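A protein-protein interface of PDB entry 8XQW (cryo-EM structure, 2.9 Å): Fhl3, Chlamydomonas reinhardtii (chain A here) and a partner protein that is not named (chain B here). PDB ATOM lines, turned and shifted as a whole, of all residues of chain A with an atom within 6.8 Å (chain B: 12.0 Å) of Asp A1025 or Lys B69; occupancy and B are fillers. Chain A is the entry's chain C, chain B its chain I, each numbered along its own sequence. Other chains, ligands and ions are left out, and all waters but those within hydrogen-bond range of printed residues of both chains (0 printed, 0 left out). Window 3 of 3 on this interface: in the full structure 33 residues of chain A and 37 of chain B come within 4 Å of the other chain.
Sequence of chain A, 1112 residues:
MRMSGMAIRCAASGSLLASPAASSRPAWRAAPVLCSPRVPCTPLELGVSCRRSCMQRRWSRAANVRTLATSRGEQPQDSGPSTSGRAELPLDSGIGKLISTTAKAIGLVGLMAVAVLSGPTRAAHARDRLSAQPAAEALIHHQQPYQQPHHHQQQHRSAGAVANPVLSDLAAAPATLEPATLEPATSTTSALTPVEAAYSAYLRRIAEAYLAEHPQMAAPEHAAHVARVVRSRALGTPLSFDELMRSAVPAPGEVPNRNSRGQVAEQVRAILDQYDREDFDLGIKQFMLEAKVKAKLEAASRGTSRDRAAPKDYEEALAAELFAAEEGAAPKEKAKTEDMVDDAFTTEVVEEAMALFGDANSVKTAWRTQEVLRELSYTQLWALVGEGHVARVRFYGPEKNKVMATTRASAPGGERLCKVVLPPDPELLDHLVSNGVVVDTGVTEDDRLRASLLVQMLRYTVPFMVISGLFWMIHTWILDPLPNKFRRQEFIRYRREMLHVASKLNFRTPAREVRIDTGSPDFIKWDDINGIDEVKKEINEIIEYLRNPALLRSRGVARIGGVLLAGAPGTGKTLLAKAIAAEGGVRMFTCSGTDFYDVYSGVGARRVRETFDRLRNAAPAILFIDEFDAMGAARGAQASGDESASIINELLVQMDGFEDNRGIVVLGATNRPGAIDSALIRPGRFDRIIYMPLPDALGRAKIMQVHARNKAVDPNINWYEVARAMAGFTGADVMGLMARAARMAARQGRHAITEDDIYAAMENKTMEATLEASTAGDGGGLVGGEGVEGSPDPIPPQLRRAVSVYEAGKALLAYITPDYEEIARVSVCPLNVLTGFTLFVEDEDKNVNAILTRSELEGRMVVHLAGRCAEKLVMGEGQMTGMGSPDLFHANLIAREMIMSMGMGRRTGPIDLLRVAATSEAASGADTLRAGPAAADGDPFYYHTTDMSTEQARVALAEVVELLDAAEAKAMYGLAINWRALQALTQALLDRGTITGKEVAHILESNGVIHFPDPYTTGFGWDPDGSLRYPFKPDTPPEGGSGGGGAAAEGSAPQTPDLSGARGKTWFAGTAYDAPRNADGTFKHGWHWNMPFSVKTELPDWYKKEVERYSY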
ATOM      1  N   TRP A1022      19.419  -9.488   3.297  1.00  0.00           N
ATOM      2  CA  TRP A1022      19.940 -10.780   2.898  1.00  0.00           C
ATOM      3  C   TRP A1022      18.954 -11.460   1.968  1.00  0.00           C
ATOM      4  O   TRP A1022      17.747 -11.422   2.206  1.00  0.00           O
ATOM      5  CB  TRP A1022      20.201 -11.656   4.114  1.00  0.00           C
ATOM      6  CG  TRP A1022      21.202 -11.092   5.017  1.00  0.00           C
ATOM      7  CD1 TRP A1022      20.972 -10.345   6.115  1.00  0.00           C
ATOM      8  CD2 TRP A1022      22.612 -11.221   4.906  1.00  0.00           C
ATOM      9  NE1 TRP A1022      22.150 -10.002   6.708  1.00  0.00           N
ATOM     10  CE2 TRP A1022      23.177 -10.527   5.975  1.00  0.00           C
ATOM     11  CE3 TRP A1022      23.454 -11.859   4.001  1.00  0.00           C
ATOM     12  CZ2 TRP A1022      24.536 -10.454   6.166  1.00  0.00           C
ATOM     13  CZ3 TRP A1022      24.793 -11.783   4.194  1.00  0.00           C
ATOM     14  CH2 TRP A1022      25.328 -11.088   5.264  1.00  0.00           C
ATOM     15  N   ASP A1023      19.467 -12.070   0.915  1.00  0.00           N
ATOM     16  CA  ASP A1023      18.618 -12.805   0.004  1.00  0.00           C
ATOM     17  C   ASP A1023      18.235 -14.147   0.619  1.00  0.00           C
ATOM     18  O   ASP A1023      18.901 -14.625   1.537  1.00  0.00           O
ATOM     19  CB  ASP A1023      19.331 -13.015  -1.323  1.00  0.00           C
ATOM     20  CG  ASP A1023      19.310 -11.782  -2.190  1.00  0.00           C
ATOM     21  OD1 ASP A1023      18.344 -11.002  -2.086  1.00  0.00           O
ATOM     22  OD2 ASP A1023      20.258 -11.588  -2.979  1.00  0.00           O
ATOM     23  N   PRO A1024      17.156 -14.770   0.147  1.00  0.00           N
ATOM     24  CA  PRO A1024      16.726 -16.038   0.754  1.00  0.00           C
ATOM     25  C   PRO A1024      17.692 -17.185   0.534  1.00  0.00           C
ATOM     26  O   PRO A1024      17.627 -18.173   1.272  1.00  0.00           O
ATOM     27  CB  PRO A1024      15.377 -16.309   0.081  1.00  0.00           C
ATOM     28  CG  PRO A1024      15.416 -15.517  -1.167  1.00  0.00           C
ATOM     29  CD  PRO A1024      16.188 -14.291  -0.849  1.00  0.00           C
ATOM     30  N   ASP A1025      18.582 -17.096  -0.447  1.00  0.00           N
ATOM     31  CA  ASP A1025      19.623 -18.098  -0.615  1.00  0.00           C
ATOM     32  C   ASP A1025      20.864 -17.794   0.206  1.00  0.00           C
ATOM     33  O   ASP A1025      21.802 -18.593   0.203  1.00  0.00           O
ATOM     34  CB  ASP A1025      20.005 -18.223  -2.087  1.00  0.00           C
ATOM     35  CG  ASP A1025      20.346 -16.896  -2.706  1.00  0.00           C
ATOM     36  OD1 ASP A1025      19.559 -15.946  -2.532  1.00  0.00           O
ATOM     37  OD2 ASP A1025      21.401 -16.795  -3.362  1.00  0.00           O
ATOM     38  N   GLY A1026      20.896 -16.664   0.898  1.00  0.00           N
ATOM     39  CA  GLY A1026      21.986 -16.335   1.781  1.00  0.00           C
ATOM     40  C   GLY A1026      22.856 -15.177   1.361  1.00  0.00           C
ATOM     41  O   GLY A1026      23.637 -14.694   2.181  1.00  0.00           O
ATOM     42  N   SER A1027      22.737 -14.700   0.131  1.00  0.00           N
ATOM     43  CA  SER A1027      23.666 -13.721  -0.402  1.00  0.00           C
ATOM     44  C   SER A1027      23.268 -12.313   0.005  1.00  0.00           C
ATOM     45  O   SER A1027      22.088 -12.003   0.156  1.00  0.00           O
ATOM     46  CB  SER A1027      23.735 -13.809  -1.922  1.00  0.00           C
ATOM     47  OG  SER A1027      23.629 -15.150  -2.352  1.00  0.00           O
ATOM     48  N   ALA B  64      31.072  -9.014  -2.779  1.00  0.00           N
ATOM     49  CA  ALA B  64      29.865  -9.427  -3.474  1.00  0.00           C
ATOM     50  C   ALA B  64      29.468 -10.834  -3.067  1.00  0.00           C
ATOM     51  O   ALA B  64      28.280 -11.134  -2.918  1.00  0.00           O
ATOM     52  CB  ALA B  64      30.068  -9.340  -4.982  1.00  0.00           C
ATOM     53  N   SER B  65      30.445 -11.713  -2.881  1.00  0.00           N
ATOM     54  CA  SER B  65      30.159 -13.106  -2.557  1.00  0.00           C
ATOM     55  C   SER B  65      30.206 -13.377  -1.057  1.00  0.00           C
ATOM     56  O   SER B  65      30.836 -14.332  -0.614  1.00  0.00           O
ATOM     57  CB  SER B  65      31.135 -14.007  -3.295  1.00  0.00           C
ATOM     58  OG  SER B  65      32.423 -13.916  -2.715  1.00  0.00           O
ATOM     59  N   ILE B  66      29.522 -12.566  -0.260  1.00  0.00           N
ATOM     60  CA  ILE B  66      29.365 -12.825   1.166  1.00  0.00           C
ATOM     61  C   ILE B  66      28.026 -13.511   1.349  1.00  0.00           C
ATOM     62  O   ILE B  66      27.000 -13.016   0.872  1.00  0.00           O
ATOM     63  CB  ILE B  66      29.435 -11.537   1.994  1.00  0.00           C
ATOM     64  CG1 ILE B  66      30.870 -11.054   2.123  1.00  0.00           C
ATOM     65  CG2 ILE B  66      28.894 -11.785   3.367  1.00  0.00           C
ATOM     66  CD1 ILE B  66      31.001  -9.822   2.960  1.00  0.00           C
ATOM     67  N   ASN B  67      28.023 -14.649   2.029  1.00  0.00           N
ATOM     68  CA  ASN B  67      26.840 -15.486   2.128  1.00  0.00           C
ATOM     69  C   ASN B  67      26.699 -16.011   3.545  1.00  0.00           C
ATOM     70  O   ASN B  67      27.553 -16.761   4.016  1.00  0.00           O
ATOM     71  CB  ASN B  67      26.932 -16.636   1.138  1.00  0.00           C
ATOM     72  CG  ASN B  67      25.755 -17.539   1.207  1.00  0.00           C
ATOM     73  OD1 ASN B  67      25.640 -18.348   2.116  1.00  0.00           O
ATOM     74  ND2 ASN B  67      24.861 -17.412   0.247  1.00  0.00           N
ATOM     75  N   ARG B  68      25.612 -15.636   4.210  1.00  0.00           N
ATOM     76  CA  ARG B  68      25.461 -15.986   5.614  1.00  0.00           C
ATOM     77  C   ARG B  68      25.017 -17.423   5.809  1.00  0.00           C
ATOM     78  O   ARG B  68      25.027 -17.918   6.937  1.00  0.00           O
ATOM     79  CB  ARG B  68      24.467 -15.049   6.284  1.00  0.00           C
ATOM     80  CG  ARG B  68      23.050 -15.305   5.900  1.00  0.00           C
ATOM     81  CD  ARG B  68      22.114 -14.816   6.964  1.00  0.00           C
ATOM     82  NE  ARG B  68      20.754 -14.708   6.472  1.00  0.00           N
ATOM     83  CZ  ARG B  68      19.825 -13.963   7.051  1.00  0.00           C
ATOM     84  NH1 ARG B  68      18.604 -13.915   6.553  1.00  0.00           N
ATOM     85  NH2 ARG B  68      20.124 -13.271   8.131  1.00  0.00           N
ATOM     86  N   LYS B  69      24.622 -18.106   4.740  1.00  0.00           N
ATOM     87  CA  LYS B  69      24.247 -19.507   4.863  1.00  0.00           C
ATOM     88  C   LYS B  69      25.473 -20.399   4.948  1.00  0.00           C
ATOM     89  O   LYS B  69      25.553 -21.275   5.813  1.00  0.00           O
ATOM     90  CB  LYS B  69      23.383 -19.929   3.684  1.00  0.00           C
ATOM     91  CG  LYS B  69      21.931 -20.084   4.012  1.00  0.00           C
ATOM     92  CD  LYS B  69      21.293 -21.072   3.068  1.00  0.00           C
ATOM     93  CE  LYS B  69      19.857 -21.339   3.450  1.00  0.00           C
ATOM     94  NZ  LYS B  69      19.226 -22.336   2.549  1.00  0.00           N
ATOM     95  N   THR B  70      26.430 -20.199   4.053  1.00  0.00           N
ATOM     96  CA  THR B  70      27.635 -21.010   4.047  1.00  0.00           C
ATOM     97  C   THR B  70      28.751 -20.423   4.889  1.00  0.00           C
ATOM     98  O   THR B  70      29.911 -20.776   4.672  1.00  0.00           O
ATOM     99  CB  THR B  70      28.127 -21.199   2.617  1.00  0.00           C
ATOM    100  OG1 THR B  70      28.984 -20.109   2.266  1.00  0.00           O
ATOM    101  CG2 THR B  70      26.954 -21.236   1.660  1.00  0.00           C
ATOM    102  N   GLY B  71      28.446 -19.532   5.821  1.00  0.00           N
ATOM    103  CA  GLY B  71      29.465 -18.976   6.684  1.00  0.00           C
ATOM    104  C   GLY B  71      30.001 -17.647   6.206  1.00  0.00           C
ATOM    105  O   GLY B  71      30.248 -17.458   5.013  1.00  0.00           O
ATOM    106  N   ILE B  72      30.184 -16.716   7.132  1.00  0.00           N
ATOM    107  CA  ILE B  72      30.758 -15.418   6.811  1.00  0.00           C
ATOM    108  C   ILE B  72      32.260 -15.474   7.041  1.00  0.00           C
ATOM    109  O   ILE B  72      32.718 -15.933   8.092  1.00  0.00           O
ATOM    110  CB  ILE B  72      30.112 -14.323   7.667  1.00  0.00           C
ATOM    111  CG1 ILE B  72      28.762 -13.930   7.090  1.00  0.00           C
ATOM    112  CG2 ILE B  72      31.003 -13.127   7.748  1.00  0.00           C
ATOM    113  CD1 ILE B  72      27.945 -13.098   8.020  1.00  0.00           C
ATOM    114  N   ARG B  73      33.035 -15.012   6.067  1.00  0.00           N
ATOM    115  CA  ARG B  73      34.479 -15.037   6.229  1.00  0.00           C
ATOM    116  C   ARG B  73      35.114 -13.962   5.369  1.00  0.00           C
ATOM    117  O   ARG B  73      34.572 -13.594   4.328  1.00  0.00           O
ATOM    118  CB  ARG B  73      35.054 -16.404   5.866  1.00  0.00           C
ATOM    119  CG  ARG B  73      34.766 -16.835   4.457  1.00  0.00           C
ATOM    120  CD  ARG B  73      35.521 -18.095   4.144  1.00  0.00           C
ATOM    121  NE  ARG B  73      35.461 -19.020   5.264  1.00  0.00           N
ATOM    122  CZ  ARG B  73      34.546 -19.971   5.394  1.00  0.00           C
ATOM    123  NH1 ARG B  73      34.562 -20.773   6.448  1.00  0.00           N
ATOM    124  NH2 ARG B  73      33.611 -20.119   4.468  1.00  0.00           N
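Among the printed residues, pairs that only touch across the chains: Trp A1022 with Arg B68, Asp A1025 with Lys B69, Gly A1026 with Ile B66, Gly A1026 with Asn B67 and Ser A1027 with Ile B66.
The backbone NH (N) of Thr B70 sits at hydrogen-bond distance from the side-chain amide oxygen (OD1) of Asn B67, 2.8 Å away. The side-chain amide oxygen (OD1) of Asn B67 lies within hydrogen-bond range of the backbone NH (N) of Lys B69 (2.8 Å). OG of Ser A1027 sits at hydrogen-bond distance from OD2 of Asp A1025 (2.9 Å).
Of the 6 printed residues of chain A, 4 touch a printed residue of chain B. Among the printed residues, no Asp or Glu carboxylate lies within 4 Å of a Lys or Arg side-chain nitrogen of the other chain.
ND2 of Asn B67 lies within hydrogen-bond range of O of Asp A1025 (3.3 Å). N of Ser A1027 lies close to ND2 of Asn B67, 3.4 Å away. O of Gly A1026 sits at hydrogen-bond distance from N of Arg B68 (3.0 Å).
Of the printed residues of chain B, Trp A1022 touches Arg B68. No residue of chain B comes within 4 Å of Asp A1023. No residue of chain B comes within 4 Å of Pro A1024. Of chain B, only Asn B67 and Lys B69 come within 4 Å of Asp A1025. Gly A1026 touches just these residues of chain B: Ile B66, Asn B67 and Arg B68. Of chain B, only Ile B66 and Asn B67 come within 4 Å of Ser A1027. Printed residues of chain A within 4 Å of Ile B66: Gly A1026 (3.98 Å) and Ser A1027 (3.6 Å). Printed residues of chain A within 4 Å of Asn B67: Asp A1025, Gly A1026 and Ser A1027. Of the printed residues of chain A, Arg B68 touches Trp A1022 (3.7 Å) and Gly A1026 (3.0 Å). Lys B69 touches one residue of chain A. The nearest residue of chain A that does not touch Lys B69 is Gly A1026 (4.3 Å).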
